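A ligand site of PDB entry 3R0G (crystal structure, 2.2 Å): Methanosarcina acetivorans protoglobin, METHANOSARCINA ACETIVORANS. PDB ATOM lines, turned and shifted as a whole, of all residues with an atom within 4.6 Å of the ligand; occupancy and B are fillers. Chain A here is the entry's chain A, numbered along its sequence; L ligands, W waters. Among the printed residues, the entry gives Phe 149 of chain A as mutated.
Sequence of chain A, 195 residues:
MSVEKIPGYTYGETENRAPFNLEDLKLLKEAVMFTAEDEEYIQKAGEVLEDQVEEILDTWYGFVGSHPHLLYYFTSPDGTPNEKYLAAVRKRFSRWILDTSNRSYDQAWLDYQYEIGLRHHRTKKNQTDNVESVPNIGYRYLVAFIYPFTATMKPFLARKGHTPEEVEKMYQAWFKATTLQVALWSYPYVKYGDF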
ATOM      1  N   VAL A  64      29.045 -12.568  23.505  1.00  0.00           N
ATOM      2  CA  VAL A  64      28.863 -11.140  23.214  1.00  0.00           C
ATOM      3  C   VAL A  64      29.934 -10.265  23.886  1.00  0.00           C
ATOM      4  O   VAL A  64      30.266  -9.166  23.391  1.00  0.00           O
ATOM      5  CB  VAL A  64      27.459 -10.674  23.669  1.00  0.00           C
ATOM      6  CG1 VAL A  64      27.330  -9.156  23.635  1.00  0.00           C
ATOM      7  CG2 VAL A  64      26.383 -11.321  22.813  1.00  0.00           C
ATOM      8  N   LEU A  70      30.977  -6.623  19.441  1.00  0.00           N
ATOM      9  CA  LEU A  70      29.668  -7.154  19.769  1.00  0.00           C
ATOM     10  C   LEU A  70      29.079  -6.601  21.083  1.00  0.00           C
ATOM     11  O   LEU A  70      27.907  -6.209  21.133  1.00  0.00           O
ATOM     12  CB  LEU A  70      29.715  -8.691  19.837  1.00  0.00           C
ATOM     13  CG  LEU A  70      30.246  -9.447  18.604  1.00  0.00           C
ATOM     14  CD1 LEU A  70      30.241 -10.962  18.865  1.00  0.00           C
ATOM     15  CD2 LEU A  70      29.445  -9.081  17.354  1.00  0.00           C
ATOM     16  N   TYR A  73      27.124  -3.077  21.261  1.00  0.00           N
ATOM     17  CA  TYR A  73      25.696  -2.746  21.121  1.00  0.00           C
ATOM     18  C   TYR A  73      24.939  -2.678  22.460  1.00  0.00           C
ATOM     19  O   TYR A  73      23.777  -2.309  22.503  1.00  0.00           O
ATOM     20  CB  TYR A  73      25.009  -3.679  20.110  1.00  0.00           C
ATOM     21  CG  TYR A  73      25.653  -3.620  18.742  1.00  0.00           C
ATOM     22  CD1 TYR A  73      25.379  -2.567  17.868  1.00  0.00           C
ATOM     23  CD2 TYR A  73      26.565  -4.600  18.329  1.00  0.00           C
ATOM     24  CE1 TYR A  73      25.983  -2.485  16.627  1.00  0.00           C
ATOM     25  CE2 TYR A  73      27.173  -4.534  17.070  1.00  0.00           C
ATOM     26  CZ  TYR A  73      26.872  -3.462  16.235  1.00  0.00           C
ATOM     27  OH  TYR A  73      27.446  -3.348  14.981  1.00  0.00           O
ATOM     28  N   PHE A  74      25.624  -3.045  23.538  1.00  0.00           N
ATOM     29  CA  PHE A  74      25.108  -2.867  24.906  1.00  0.00           C
ATOM     30  C   PHE A  74      25.697  -1.680  25.681  1.00  0.00           C
ATOM     31  O   PHE A  74      25.311  -1.443  26.820  1.00  0.00           O
ATOM     32  CB  PHE A  74      25.292  -4.146  25.722  1.00  0.00           C
ATOM     33  CG  PHE A  74      24.324  -5.232  25.372  1.00  0.00           C
ATOM     34  CD1 PHE A  74      23.032  -5.224  25.900  1.00  0.00           C
ATOM     35  CD2 PHE A  74      24.680  -6.238  24.476  1.00  0.00           C
ATOM     36  CE1 PHE A  74      22.128  -6.205  25.557  1.00  0.00           C
ATOM     37  CE2 PHE A  74      23.787  -7.228  24.132  1.00  0.00           C
ATOM     38  CZ  PHE A  74      22.507  -7.216  24.664  1.00  0.00           C
ATOM     39  N   TYR A  85      20.916  -2.179  31.077  1.00  0.00           N
ATOM     40  CA  TYR A  85      20.494  -2.609  29.741  1.00  0.00           C
ATOM     41  C   TYR A  85      20.607  -4.126  29.603  1.00  0.00           C
ATOM     42  O   TYR A  85      19.689  -4.796  29.137  1.00  0.00           O
ATOM     43  CB  TYR A  85      21.438  -1.972  28.747  1.00  0.00           C
ATOM     44  CG  TYR A  85      20.966  -1.896  27.311  1.00  0.00           C
ATOM     45  CD1 TYR A  85      19.664  -2.184  26.955  1.00  0.00           C
ATOM     46  CD2 TYR A  85      21.849  -1.533  26.315  1.00  0.00           C
ATOM     47  CE1 TYR A  85      19.259  -2.108  25.631  1.00  0.00           C
ATOM     48  CE2 TYR A  85      21.466  -1.452  24.991  1.00  0.00           C
ATOM     49  CZ  TYR A  85      20.184  -1.729  24.656  1.00  0.00           C
ATOM     50  OH  TYR A  85      19.851  -1.628  23.323  1.00  0.00           O
ATOM     51  N   VAL A  89      17.522  -6.774  29.312  1.00  0.00           N
ATOM     52  CA  VAL A  89      17.440  -7.559  28.099  1.00  0.00           C
ATOM     53  C   VAL A  89      17.524  -9.059  28.408  1.00  0.00           C
ATOM     54  O   VAL A  89      16.792  -9.866  27.824  1.00  0.00           O
ATOM     55  CB  VAL A  89      18.517  -7.162  27.071  1.00  0.00           C
ATOM     56  CG1 VAL A  89      18.664  -8.252  26.011  1.00  0.00           C
ATOM     57  CG2 VAL A  89      18.148  -5.827  26.385  1.00  0.00           C
ATOM     58  N   ARG A  92      14.040 -10.758  29.189  1.00  0.00           N
ATOM     59  CA  ARG A  92      13.230 -10.991  27.999  1.00  0.00           C
ATOM     60  C   ARG A  92      13.770 -12.121  27.123  1.00  0.00           C
ATOM     61  O   ARG A  92      13.019 -12.940  26.612  1.00  0.00           O
ATOM     62  CB  ARG A  92      13.063  -9.682  27.197  1.00  0.00           C
ATOM     63  CG  ARG A  92      12.449  -8.551  28.036  1.00  0.00           C
ATOM     64  CD  ARG A  92      11.796  -7.404  27.220  1.00  0.00           C
ATOM     65  NE  ARG A  92      12.822  -6.603  26.579  1.00  0.00           N
ATOM     66  CZ  ARG A  92      13.544  -5.650  27.184  1.00  0.00           C
ATOM     67  NH1 ARG A  92      13.333  -5.344  28.463  1.00  0.00           N
ATOM     68  NH2 ARG A  92      14.478  -5.008  26.491  1.00  0.00           N
ATOM     69  N   PHE A  93      15.075 -12.160  26.936  1.00  0.00           N
ATOM     70  CA  PHE A  93      15.759 -13.244  26.247  1.00  0.00           C
ATOM     71  C   PHE A  93      15.456 -14.616  26.876  1.00  0.00           C
ATOM     72  O   PHE A  93      15.128 -15.571  26.186  1.00  0.00           O
ATOM     73  CB  PHE A  93      17.278 -12.963  26.245  1.00  0.00           C
ATOM     74  CG  PHE A  93      18.070 -13.854  25.323  1.00  0.00           C
ATOM     75  CD1 PHE A  93      18.646 -13.345  24.175  1.00  0.00           C
ATOM     76  CD2 PHE A  93      18.268 -15.194  25.638  1.00  0.00           C
ATOM     77  CE1 PHE A  93      19.372 -14.146  23.338  1.00  0.00           C
ATOM     78  CE2 PHE A  93      19.021 -16.008  24.806  1.00  0.00           C
ATOM     79  CZ  PHE A  93      19.571 -15.486  23.652  1.00  0.00           C
ATOM     80  N   TRP A  96      11.965 -15.671  25.858  1.00  0.00           N
ATOM     81  CA  TRP A  96      12.005 -16.062  24.447  1.00  0.00           C
ATOM     82  C   TRP A  96      12.478 -17.494  24.213  1.00  0.00           C
ATOM     83  O   TRP A  96      11.888 -18.215  23.406  1.00  0.00           O
ATOM     84  CB  TRP A  96      12.870 -15.083  23.679  1.00  0.00           C
ATOM     85  CG  TRP A  96      13.072 -15.423  22.242  1.00  0.00           C
ATOM     86  CD1 TRP A  96      12.284 -15.058  21.201  1.00  0.00           C
ATOM     87  CD2 TRP A  96      14.176 -16.146  21.685  1.00  0.00           C
ATOM     88  NE1 TRP A  96      12.811 -15.535  20.022  1.00  0.00           N
ATOM     89  CE2 TRP A  96      13.968 -16.199  20.293  1.00  0.00           C
ATOM     90  CE3 TRP A  96      15.305 -16.768  22.223  1.00  0.00           C
ATOM     91  CZ2 TRP A  96      14.860 -16.841  19.427  1.00  0.00           C
ATOM     92  CZ3 TRP A  96      16.194 -17.400  21.354  1.00  0.00           C
ATOM     93  CH2 TRP A  96      15.961 -17.442  19.981  1.00  0.00           C
ATOM     94  N   TYR A 112       4.935 -10.481  17.778  1.00  0.00           N
ATOM     95  CA  TYR A 112       6.036 -10.237  18.675  1.00  0.00           C
ATOM     96  C   TYR A 112       7.382 -10.431  17.980  1.00  0.00           C
ATOM     97  O   TYR A 112       8.348  -9.722  18.276  1.00  0.00           O
ATOM     98  CB  TYR A 112       5.912 -11.071  19.953  1.00  0.00           C
ATOM     99  CG  TYR A 112       6.702 -10.476  21.106  1.00  0.00           C
ATOM    100  CD1 TYR A 112       6.344  -9.242  21.662  1.00  0.00           C
ATOM    101  CD2 TYR A 112       7.814 -11.126  21.606  1.00  0.00           C
ATOM    102  CE1 TYR A 112       7.088  -8.692  22.714  1.00  0.00           C
ATOM    103  CE2 TYR A 112       8.546 -10.588  22.633  1.00  0.00           C
ATOM    104  CZ  TYR A 112       8.180  -9.376  23.191  1.00  0.00           C
ATOM    105  OH  TYR A 112       8.928  -8.865  24.223  1.00  0.00           O
ATOM    106  N   ILE A 116      10.280  -7.645  18.045  1.00  0.00           N
ATOM    107  CA  ILE A 116      11.620  -7.932  18.466  1.00  0.00           C
ATOM    108  C   ILE A 116      12.577  -7.419  17.416  1.00  0.00           C
ATOM    109  O   ILE A 116      13.633  -6.898  17.732  1.00  0.00           O
ATOM    110  CB  ILE A 116      11.828  -9.446  18.617  1.00  0.00           C
ATOM    111  CG1 ILE A 116      10.998  -9.985  19.788  1.00  0.00           C
ATOM    112  CG2 ILE A 116      13.341  -9.752  18.706  1.00  0.00           C
ATOM    113  CD1 ILE A 116      11.419 -11.363  20.279  1.00  0.00           C
ATOM    114  N   ARG A 119      13.138  -3.885  17.818  1.00  0.00           N
ATOM    115  CA  ARG A 119      13.907  -3.495  18.990  1.00  0.00           C
ATOM    116  C   ARG A 119      15.404  -3.657  18.724  1.00  0.00           C
ATOM    117  O   ARG A 119      16.239  -3.053  19.400  1.00  0.00           O
ATOM    118  CB  ARG A 119      13.450  -4.279  20.232  1.00  0.00           C
ATOM    119  CG  ARG A 119      12.035  -3.964  20.665  1.00  0.00           C
ATOM    120  CD  ARG A 119      11.641  -4.717  21.924  1.00  0.00           C
ATOM    121  NE  ARG A 119      10.263  -4.407  22.318  1.00  0.00           N
ATOM    122  CZ  ARG A 119       9.720  -4.760  23.487  1.00  0.00           C
ATOM    123  NH1 ARG A 119      10.419  -5.462  24.366  1.00  0.00           N
ATOM    124  NH2 ARG A 119       8.460  -4.431  23.760  1.00  0.00           N
ATOM    125  N   HIS A 120      15.724  -4.460  17.716  1.00  0.00           N
ATOM    126  CA  HIS A 120      17.119  -4.590  17.268  1.00  0.00           C
ATOM    127  C   HIS A 120      17.452  -3.490  16.273  1.00  0.00           C
ATOM    128  O   HIS A 120      18.546  -2.978  16.255  1.00  0.00           O
ATOM    129  CB  HIS A 120      17.349  -5.951  16.591  1.00  0.00           C
ATOM    130  CG  HIS A 120      17.558  -7.076  17.552  1.00  0.00           C
ATOM    131  ND1 HIS A 120      16.511  -7.707  18.197  1.00  0.00           N
ATOM    132  CD2 HIS A 120      18.686  -7.676  17.998  1.00  0.00           C
ATOM    133  CE1 HIS A 120      16.996  -8.640  18.993  1.00  0.00           C
ATOM    134  NE2 HIS A 120      18.306  -8.638  18.892  1.00  0.00           N
ATOM    135  N   LYS A 125      15.249   0.351  19.072  1.00  0.00           N
ATOM    136  CA  LYS A 125      16.346  -0.010  19.947  1.00  0.00           C
ATOM    137  C   LYS A 125      16.522   1.054  21.026  1.00  0.00           C
ATOM    138  O   LYS A 125      16.398   2.253  20.754  1.00  0.00           O
ATOM    139  CB  LYS A 125      17.660  -0.269  19.178  1.00  0.00           C
ATOM    140  CG  LYS A 125      18.855  -0.569  20.100  1.00  0.00           C
ATOM    141  CD  LYS A 125      20.016  -1.201  19.332  1.00  0.00           C
ATOM    142  CE  LYS A 125      21.309  -1.299  20.141  1.00  0.00           C
ATOM    143  NZ  LYS A 125      21.369  -0.402  21.348  1.00  0.00           N
ATOM    144  N   ASN A 126      16.804   0.589  22.249  1.00  0.00           N
ATOM    145  CA  ASN A 126      16.988   1.444  23.407  1.00  0.00           C
ATOM    146  C   ASN A 126      15.752   2.112  24.050  1.00  0.00           C
ATOM    147  O   ASN A 126      15.854   2.737  25.100  1.00  0.00           O
ATOM    148  CB  ASN A 126      17.939   2.635  23.099  1.00  0.00           C
ATOM    149  CG  ASN A 126      19.253   2.168  22.483  1.00  0.00           C
ATOM    150  OD1 ASN A 126      19.818   1.116  22.880  1.00  0.00           O
ATOM    151  ND2 ASN A 126      19.723   2.912  21.492  1.00  0.00           N
ATOM    152  N   THR A 128      12.770   0.508  24.891  1.00  0.00           N
ATOM    153  CA  THR A 128      12.125  -0.396  25.821  1.00  0.00           C
ATOM    154  C   THR A 128      12.615  -0.191  27.241  1.00  0.00           C
ATOM    155  O   THR A 128      11.821  -0.189  28.198  1.00  0.00           O
ATOM    156  CB  THR A 128      12.300  -1.861  25.383  1.00  0.00           C
ATOM    157  OG1 THR A 128      11.600  -2.073  24.146  1.00  0.00           O
ATOM    158  CG2 THR A 128      11.735  -2.827  26.423  1.00  0.00           C
ATOM    159  N   ASP A 129      13.914  -0.005  27.395  1.00  0.00           N
ATOM    160  CA  ASP A 129      14.509   0.154  28.705  1.00  0.00           C
ATOM    161  C   ASP A 129      14.919   1.581  29.012  1.00  0.00           C
ATOM    162  O   ASP A 129      15.507   1.850  30.049  1.00  0.00           O
ATOM    163  CB  ASP A 129      15.693  -0.795  28.854  1.00  0.00           C
ATOM    164  CG  ASP A 129      15.359  -2.168  28.369  1.00  0.00           C
ATOM    165  OD1 ASP A 129      14.452  -2.773  28.962  1.00  0.00           O
ATOM    166  OD2 ASP A 129      15.973  -2.629  27.369  1.00  0.00           O
ATOM    167  N   ILE A 137      21.712  -1.926  15.603  1.00  0.00           N
ATOM    168  CA  ILE A 137      22.544  -3.133  15.496  1.00  0.00           C
ATOM    169  C   ILE A 137      22.577  -3.536  14.022  1.00  0.00           C
ATOM    170  O   ILE A 137      21.553  -3.854  13.457  1.00  0.00           O
ATOM    171  CB  ILE A 137      21.973  -4.328  16.286  1.00  0.00           C
ATOM    172  CG1 ILE A 137      21.638  -3.913  17.714  1.00  0.00           C
ATOM    173  CG2 ILE A 137      22.919  -5.490  16.261  1.00  0.00           C
ATOM    174  CD1 ILE A 137      20.809  -4.925  18.457  1.00  0.00           C
ATOM    175  N   TYR A 141      25.062  -8.786  11.720  1.00  0.00           N
ATOM    176  CA  TYR A 141      25.322  -9.577  12.923  1.00  0.00           C
ATOM    177  C   TYR A 141      24.102 -10.410  13.323  1.00  0.00           C
ATOM    178  O   TYR A 141      24.242 -11.499  13.871  1.00  0.00           O
ATOM    179  CB  TYR A 141      25.792  -8.689  14.078  1.00  0.00           C
ATOM    180  CG  TYR A 141      27.168  -8.082  13.828  1.00  0.00           C
ATOM    181  CD1 TYR A 141      28.272  -8.886  13.604  1.00  0.00           C
ATOM    182  CD2 TYR A 141      27.337  -6.708  13.770  1.00  0.00           C
ATOM    183  CE1 TYR A 141      29.523  -8.337  13.366  1.00  0.00           C
ATOM    184  CE2 TYR A 141      28.571  -6.145  13.522  1.00  0.00           C
ATOM    185  CZ  TYR A 141      29.654  -6.956  13.322  1.00  0.00           C
ATOM    186  OH  TYR A 141      30.886  -6.384  13.071  1.00  0.00           O
ATOM    187  N   LEU A 142      22.911  -9.902  13.031  1.00  0.00           N
ATOM    188  CA  LEU A 142      21.672 -10.623  13.294  1.00  0.00           C
ATOM    189  C   LEU A 142      21.719 -11.973  12.587  1.00  0.00           C
ATOM    190  O   LEU A 142      21.453 -13.027  13.199  1.00  0.00           O
ATOM    191  CB  LEU A 142      20.472  -9.810  12.796  1.00  0.00           C
ATOM    192  CG  LEU A 142      19.671  -9.030  13.844  1.00  0.00           C
ATOM    193  CD1 LEU A 142      20.399  -7.740  14.258  1.00  0.00           C
ATOM    194  CD2 LEU A 142      18.252  -8.703  13.310  1.00  0.00           C
ATOM    195  N   PHE A 145      24.692 -14.230  13.939  1.00  0.00           N
ATOM    196  CA  PHE A 145      24.346 -14.832  15.226  1.00  0.00           C
ATOM    197  C   PHE A 145      23.522 -16.138  15.208  1.00  0.00           C
ATOM    198  O   PHE A 145      23.498 -16.863  16.201  1.00  0.00           O
ATOM    199  CB  PHE A 145      23.676 -13.793  16.120  1.00  0.00           C
ATOM    200  CG  PHE A 145      24.649 -12.999  16.969  1.00  0.00           C
ATOM    201  CD1 PHE A 145      25.921 -12.693  16.487  1.00  0.00           C
ATOM    202  CD2 PHE A 145      24.289 -12.584  18.230  1.00  0.00           C
ATOM    203  CE1 PHE A 145      26.804 -11.971  17.254  1.00  0.00           C
ATOM    204  CE2 PHE A 145      25.170 -11.874  18.992  1.00  0.00           C
ATOM    205  CZ  PHE A 145      26.430 -11.559  18.511  1.00  0.00           C
ATOM    206  N   ILE A 146      22.830 -16.416  14.092  1.00  0.00           N
ATOM    207  CA  ILE A 146      22.228 -17.727  13.844  1.00  0.00           C
ATOM    208  C   ILE A 146      23.179 -18.885  14.171  1.00  0.00           C
ATOM    209  O   ILE A 146      22.763 -19.847  14.809  1.00  0.00           O
ATOM    210  CB  ILE A 146      21.736 -17.905  12.377  1.00  0.00           C
ATOM    211  CG1 ILE A 146      20.636 -16.878  12.022  1.00  0.00           C
ATOM    212  CG2 ILE A 146      21.252 -19.366  12.119  1.00  0.00           C
ATOM    213  CD1 ILE A 146      20.200 -16.894  10.576  1.00  0.00           C
ATOM    214  N   PHE A 149      24.143 -18.954  18.150  1.00  0.00           N
ATOM    215  CA  PHE A 149      22.988 -19.305  18.956  1.00  0.00           C
ATOM    216  C   PHE A 149      22.630 -20.770  18.820  1.00  0.00           C
ATOM    217  O   PHE A 149      22.472 -21.471  19.816  1.00  0.00           O
ATOM    218  CB  PHE A 149      21.757 -18.465  18.651  1.00  0.00           C
ATOM    219  CG  PHE A 149      20.545 -18.888  19.444  1.00  0.00           C
ATOM    220  CD1 PHE A 149      20.435 -18.578  20.793  1.00  0.00           C
ATOM    221  CD2 PHE A 149      19.531 -19.628  18.840  1.00  0.00           C
ATOM    222  CE1 PHE A 149      19.327 -18.976  21.527  1.00  0.00           C
ATOM    223  CE2 PHE A 149      18.407 -20.021  19.567  1.00  0.00           C
ATOM    224  CZ  PHE A 149      18.308 -19.698  20.917  1.00  0.00           C
ATOM    225  N   THR A 178      15.195 -20.814  14.973  1.00  0.00           N
ATOM    226  CA  THR A 178      16.087 -19.680  15.015  1.00  0.00           C
ATOM    227  C   THR A 178      16.160 -18.977  13.640  1.00  0.00           C
ATOM    228  O   THR A 178      15.894 -17.765  13.534  1.00  0.00           O
ATOM    229  CB  THR A 178      17.494 -20.080  15.469  1.00  0.00           C
ATOM    230  OG1 THR A 178      17.416 -20.771  16.721  1.00  0.00           O
ATOM    231  CG2 THR A 178      18.395 -18.858  15.633  1.00  0.00           C
ATOM    232  N   VAL A 182      14.907 -15.155  12.945  1.00  0.00           N
ATOM    233  CA  VAL A 182      15.789 -14.158  12.376  1.00  0.00           C
ATOM    234  C   VAL A 182      15.322 -13.657  11.007  1.00  0.00           C
ATOM    235  O   VAL A 182      15.271 -12.437  10.775  1.00  0.00           O
ATOM    236  CB  VAL A 182      17.220 -14.657  12.340  1.00  0.00           C
ATOM    237  CG1 VAL A 182      18.122 -13.617  11.659  1.00  0.00           C
ATOM    238  CG2 VAL A 182      17.710 -14.931  13.786  1.00  0.00           C
ATOM    239  N   TRP A 185      12.768 -11.174  11.621  1.00  0.00           N
ATOM    240  CA  TRP A 185      13.344  -9.949  12.170  1.00  0.00           C
ATOM    241  C   TRP A 185      13.940  -8.960  11.176  1.00  0.00           C
ATOM    242  O   TRP A 185      14.076  -7.772  11.479  1.00  0.00           O
ATOM    243  CB  TRP A 185      14.377 -10.237  13.267  1.00  0.00           C
ATOM    244  CG  TRP A 185      13.830 -11.075  14.384  1.00  0.00           C
ATOM    245  CD1 TRP A 185      12.534 -11.410  14.582  1.00  0.00           C
ATOM    246  CD2 TRP A 185      14.576 -11.672  15.443  1.00  0.00           C
ATOM    247  NE1 TRP A 185      12.417 -12.202  15.696  1.00  0.00           N
ATOM    248  CE2 TRP A 185      13.655 -12.381  16.245  1.00  0.00           C
ATOM    249  CE3 TRP A 185      15.930 -11.687  15.794  1.00  0.00           C
ATOM    250  CZ2 TRP A 185      14.036 -13.101  17.384  1.00  0.00           C
ATOM    251  CZ3 TRP A 185      16.311 -12.407  16.934  1.00  0.00           C
ATOM    252  CH2 TRP A 185      15.363 -13.101  17.705  1.00  0.00           C
HETATM  253  C1  LIG L   1      17.306  -8.108  22.332  1.00  0.00           C
HETATM  254  C2  LIG L   1      17.458 -12.651  20.623  1.00  0.00           C
HETATM  255  C3  LIG L   1      20.877 -11.126  17.560  1.00  0.00           C
HETATM  256  C4  LIG L   1      21.960  -7.727  20.888  1.00  0.00           C
HETATM  257  C5  LIG L   1      16.989  -9.438  22.117  1.00  0.00           C
HETATM  258  C6  LIG L   1      15.852 -10.162  22.679  1.00  0.00           C
HETATM  259  C7  LIG L   1      15.894 -11.412  22.203  1.00  0.00           C
HETATM  260  C8  LIG L   1      17.042 -11.534  21.318  1.00  0.00           C
HETATM  261  C9  LIG L   1      14.878 -12.540  22.548  1.00  0.00           C
HETATM  262  C10 LIG L   1      14.788  -9.598  23.659  1.00  0.00           C
HETATM  263  C11 LIG L   1      13.533  -9.286  22.843  1.00  0.00           C
HETATM  264  C12 LIG L   1      12.417  -8.747  23.692  1.00  0.00           C
HETATM  265  O1  LIG L   1      11.377  -9.420  23.866  1.00  0.00           O
HETATM  266  O2  LIG L   1      12.556  -7.602  24.180  1.00  0.00           O
HETATM  267  C13 LIG L   1      18.382 -12.671  19.590  1.00  0.00           C
HETATM  268  C14 LIG L   1      18.704 -13.753  18.685  1.00  0.00           C
HETATM  269  C15 LIG L   1      19.642 -13.339  17.831  1.00  0.00           C
HETATM  270  C16 LIG L   1      19.960 -11.966  18.169  1.00  0.00           C
HETATM  271  C17 LIG L   1      18.049 -15.150  18.726  1.00  0.00           C
HETATM  272  C18 LIG L   1      20.312 -14.134  16.672  1.00  0.00           C
HETATM  273  C19 LIG L   1      20.297 -15.473  16.571  1.00  0.00           C
HETATM  274  C20 LIG L   1      21.536 -10.114  18.251  1.00  0.00           C
HETATM  275  C21 LIG L   1      22.836  -9.561  17.929  1.00  0.00           C
HETATM  276  C22 LIG L   1      23.128  -8.636  18.839  1.00  0.00           C
HETATM  277  C23 LIG L   1      22.039  -8.564  19.792  1.00  0.00           C
HETATM  278  C24 LIG L   1      23.720  -9.956  16.717  1.00  0.00           C
HETATM  279  C25 LIG L   1      24.413  -7.795  18.893  1.00  0.00           C
HETATM  280  C26 LIG L   1      25.142  -7.854  20.014  1.00  0.00           C
HETATM  281  C27 LIG L   1      20.749  -7.352  21.451  1.00  0.00           C
HETATM  282  C28 LIG L   1      20.406  -6.065  22.023  1.00  0.00           C
HETATM  283  C29 LIG L   1      18.940  -6.186  22.451  1.00  0.00           C
HETATM  284  C30 LIG L   1      18.550  -7.525  22.106  1.00  0.00           C
HETATM  285  C31 LIG L   1      21.315  -4.817  22.160  1.00  0.00           C
HETATM  286  C32 LIG L   1      18.075  -5.092  23.136  1.00  0.00           C
HETATM  287  C33 LIG L   1      17.254  -4.391  22.052  1.00  0.00           C
HETATM  288  C34 LIG L   1      16.466  -3.257  22.672  1.00  0.00           C
HETATM  289  O3  LIG L   1      17.105  -2.187  22.918  1.00  0.00           O
HETATM  290  O4  LIG L   1      15.221  -3.454  22.949  1.00  0.00           O
HETATM  291  N1  LIG L   1      17.670 -10.300  21.292  1.00  0.00           N
HETATM  292  N2  LIG L   1      19.176 -11.597  19.240  1.00  0.00           N
HETATM  293  N3  LIG L   1      21.089  -9.491  19.386  1.00  0.00           N
HETATM  294  N4  LIG L   1      19.632  -8.178  21.515  1.00  0.00           N
HETATM  295 FE1  LIG L   1      19.351  -9.854  20.274  1.00  0.00          FE
HETATM  296  O   HOH W   1      11.212 -12.120  24.665  1.00  0.00           O
HETATM  297  O   HOH W   2      20.362 -10.760  22.862  1.00  0.00           O
HETATM  298  O   HOH W   3      15.799  -0.643  25.550  1.00  0.00           O
HETATM  299  O   HOH W   4      14.033  -1.388  22.557  1.00  0.00           O
HETATM  300  O   HOH W   5      22.585 -11.443  20.561  1.00  0.00           O
HETATM  301  O   HOH W   6      15.127  -5.859  23.773  1.00  0.00           O
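NE of Arg 92 is in salt-bridge range of O2 of the ligand, at 2.6 Å. An oxygen (O1) of the ligand lies within hydrogen-bond range of the side-chain hydroxyl of Tyr 112 (2.5 Å). O2 of the ligand is in salt-bridge range of NH1 of Arg 119, 3.0 Å away. NE2 of His 120 binds FE1 of the ligand, 2.1 Å away. The backbone NH (N) of Asn 126 is in hydrogen-bond range of an oxygen (O3) of the ligand, at 2.9 Å. O3 of the ligand is in hydrogen-bond range of OH of Tyr 85, at 2.8 Å.
OH of Tyr 85 is in hydrogen-bond range of OD1 of Asn 126, 2.8 Å away. The backbone carbonyl oxygen of His 120 is in hydrogen-bond range of the backbone NH of Ile 137 (3.4 Å). The backbone carbonyl oxygen (O) of Ile 116 sits at hydrogen-bond distance from a ring nitrogen (ND1) of His 120 (3.0 Å). The side-chain amino group (NZ) of Lys 125 lies within hydrogen-bond range of the side-chain hydroxyl (OH) of Tyr 85 (2.8 Å). The side-chain hydroxyl (OG1) of Thr 128 lies within hydrogen-bond range of the guanidinium group (NE) of Arg 119 (3.3 Å). The side-chain carboxylate (OD1) of Asp 129 is in salt-bridge range of the guanidinium group (NH1) of Arg 92, at 2.8 Å. OD1 of Asn 126 lies within hydrogen-bond range of NZ of Lys 125 (2.7 Å). NZ of Lys 125 sits at hydrogen-bond distance from O of Tyr 73, at 3.3 Å.
Residues that only touch the ligand: Phe 145 (3.1 Å), Trp 185 (3.3 Å), Tyr 141 (3.3 Å), Val 89 (3.3 Å), Trp 96 (3.3 Å), Leu 70 (3.4 Å), Tyr 73 (3.5 Å), Phe 74 (3.6 Å), Phe 93 (3.6 Å), Ile 146 (3.7 Å), Lys 125 (3.7 Å), Ile 137 (3.7 Å), Leu 142 (3.8 Å), Val 182 (3.8 Å), Ile 116 (3.9 Å), Phe 149 (3.9 Å) and Thr 178 (3.99 Å). Hydrophobic or aromatic side chains that line the ligand: Tyr 73, Phe 74, Tyr 85, Val 89, Phe 93, Trp 96, Tyr 112, Ile 116, His 120, Ile 137, Tyr 141, Phe 145, Phe 149, Val 182 and Trp 185. 23 residues have an atom within 4 Å of the ligand: Leu 70, Tyr 73, Phe 74, Tyr 85, Val 89, Arg 92, Phe 93, Trp 96, Tyr 112, Ile 116, Arg 119, His 120, Lys 125, Asn 126, Ile 137, Tyr 141, Leu 142, Phe 145, Ile 146, Phe 149, Thr 178, Val 182 and Trp 185.
Water W4 lies within hydrogen-bond range of an oxygen (O4) of the ligand, the side-chain hydroxyl of Thr 128 and the backbone NH of Asn 126. Water W6 bridges O4 of the ligand (2.5 Å) and NH2 of Arg 92 (2.9 Å). Water W1 bridges O of Arg 92 (2.8 Å) and O1 of the ligand (2.8 Å). Water W3 lies within hydrogen-bond range of OD2 of Asp 129 (2.7 Å), N of Thr 128 (3.3 Å), O3 of the ligand (3.3 Å) and O of Asn 126 (3.4 Å).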
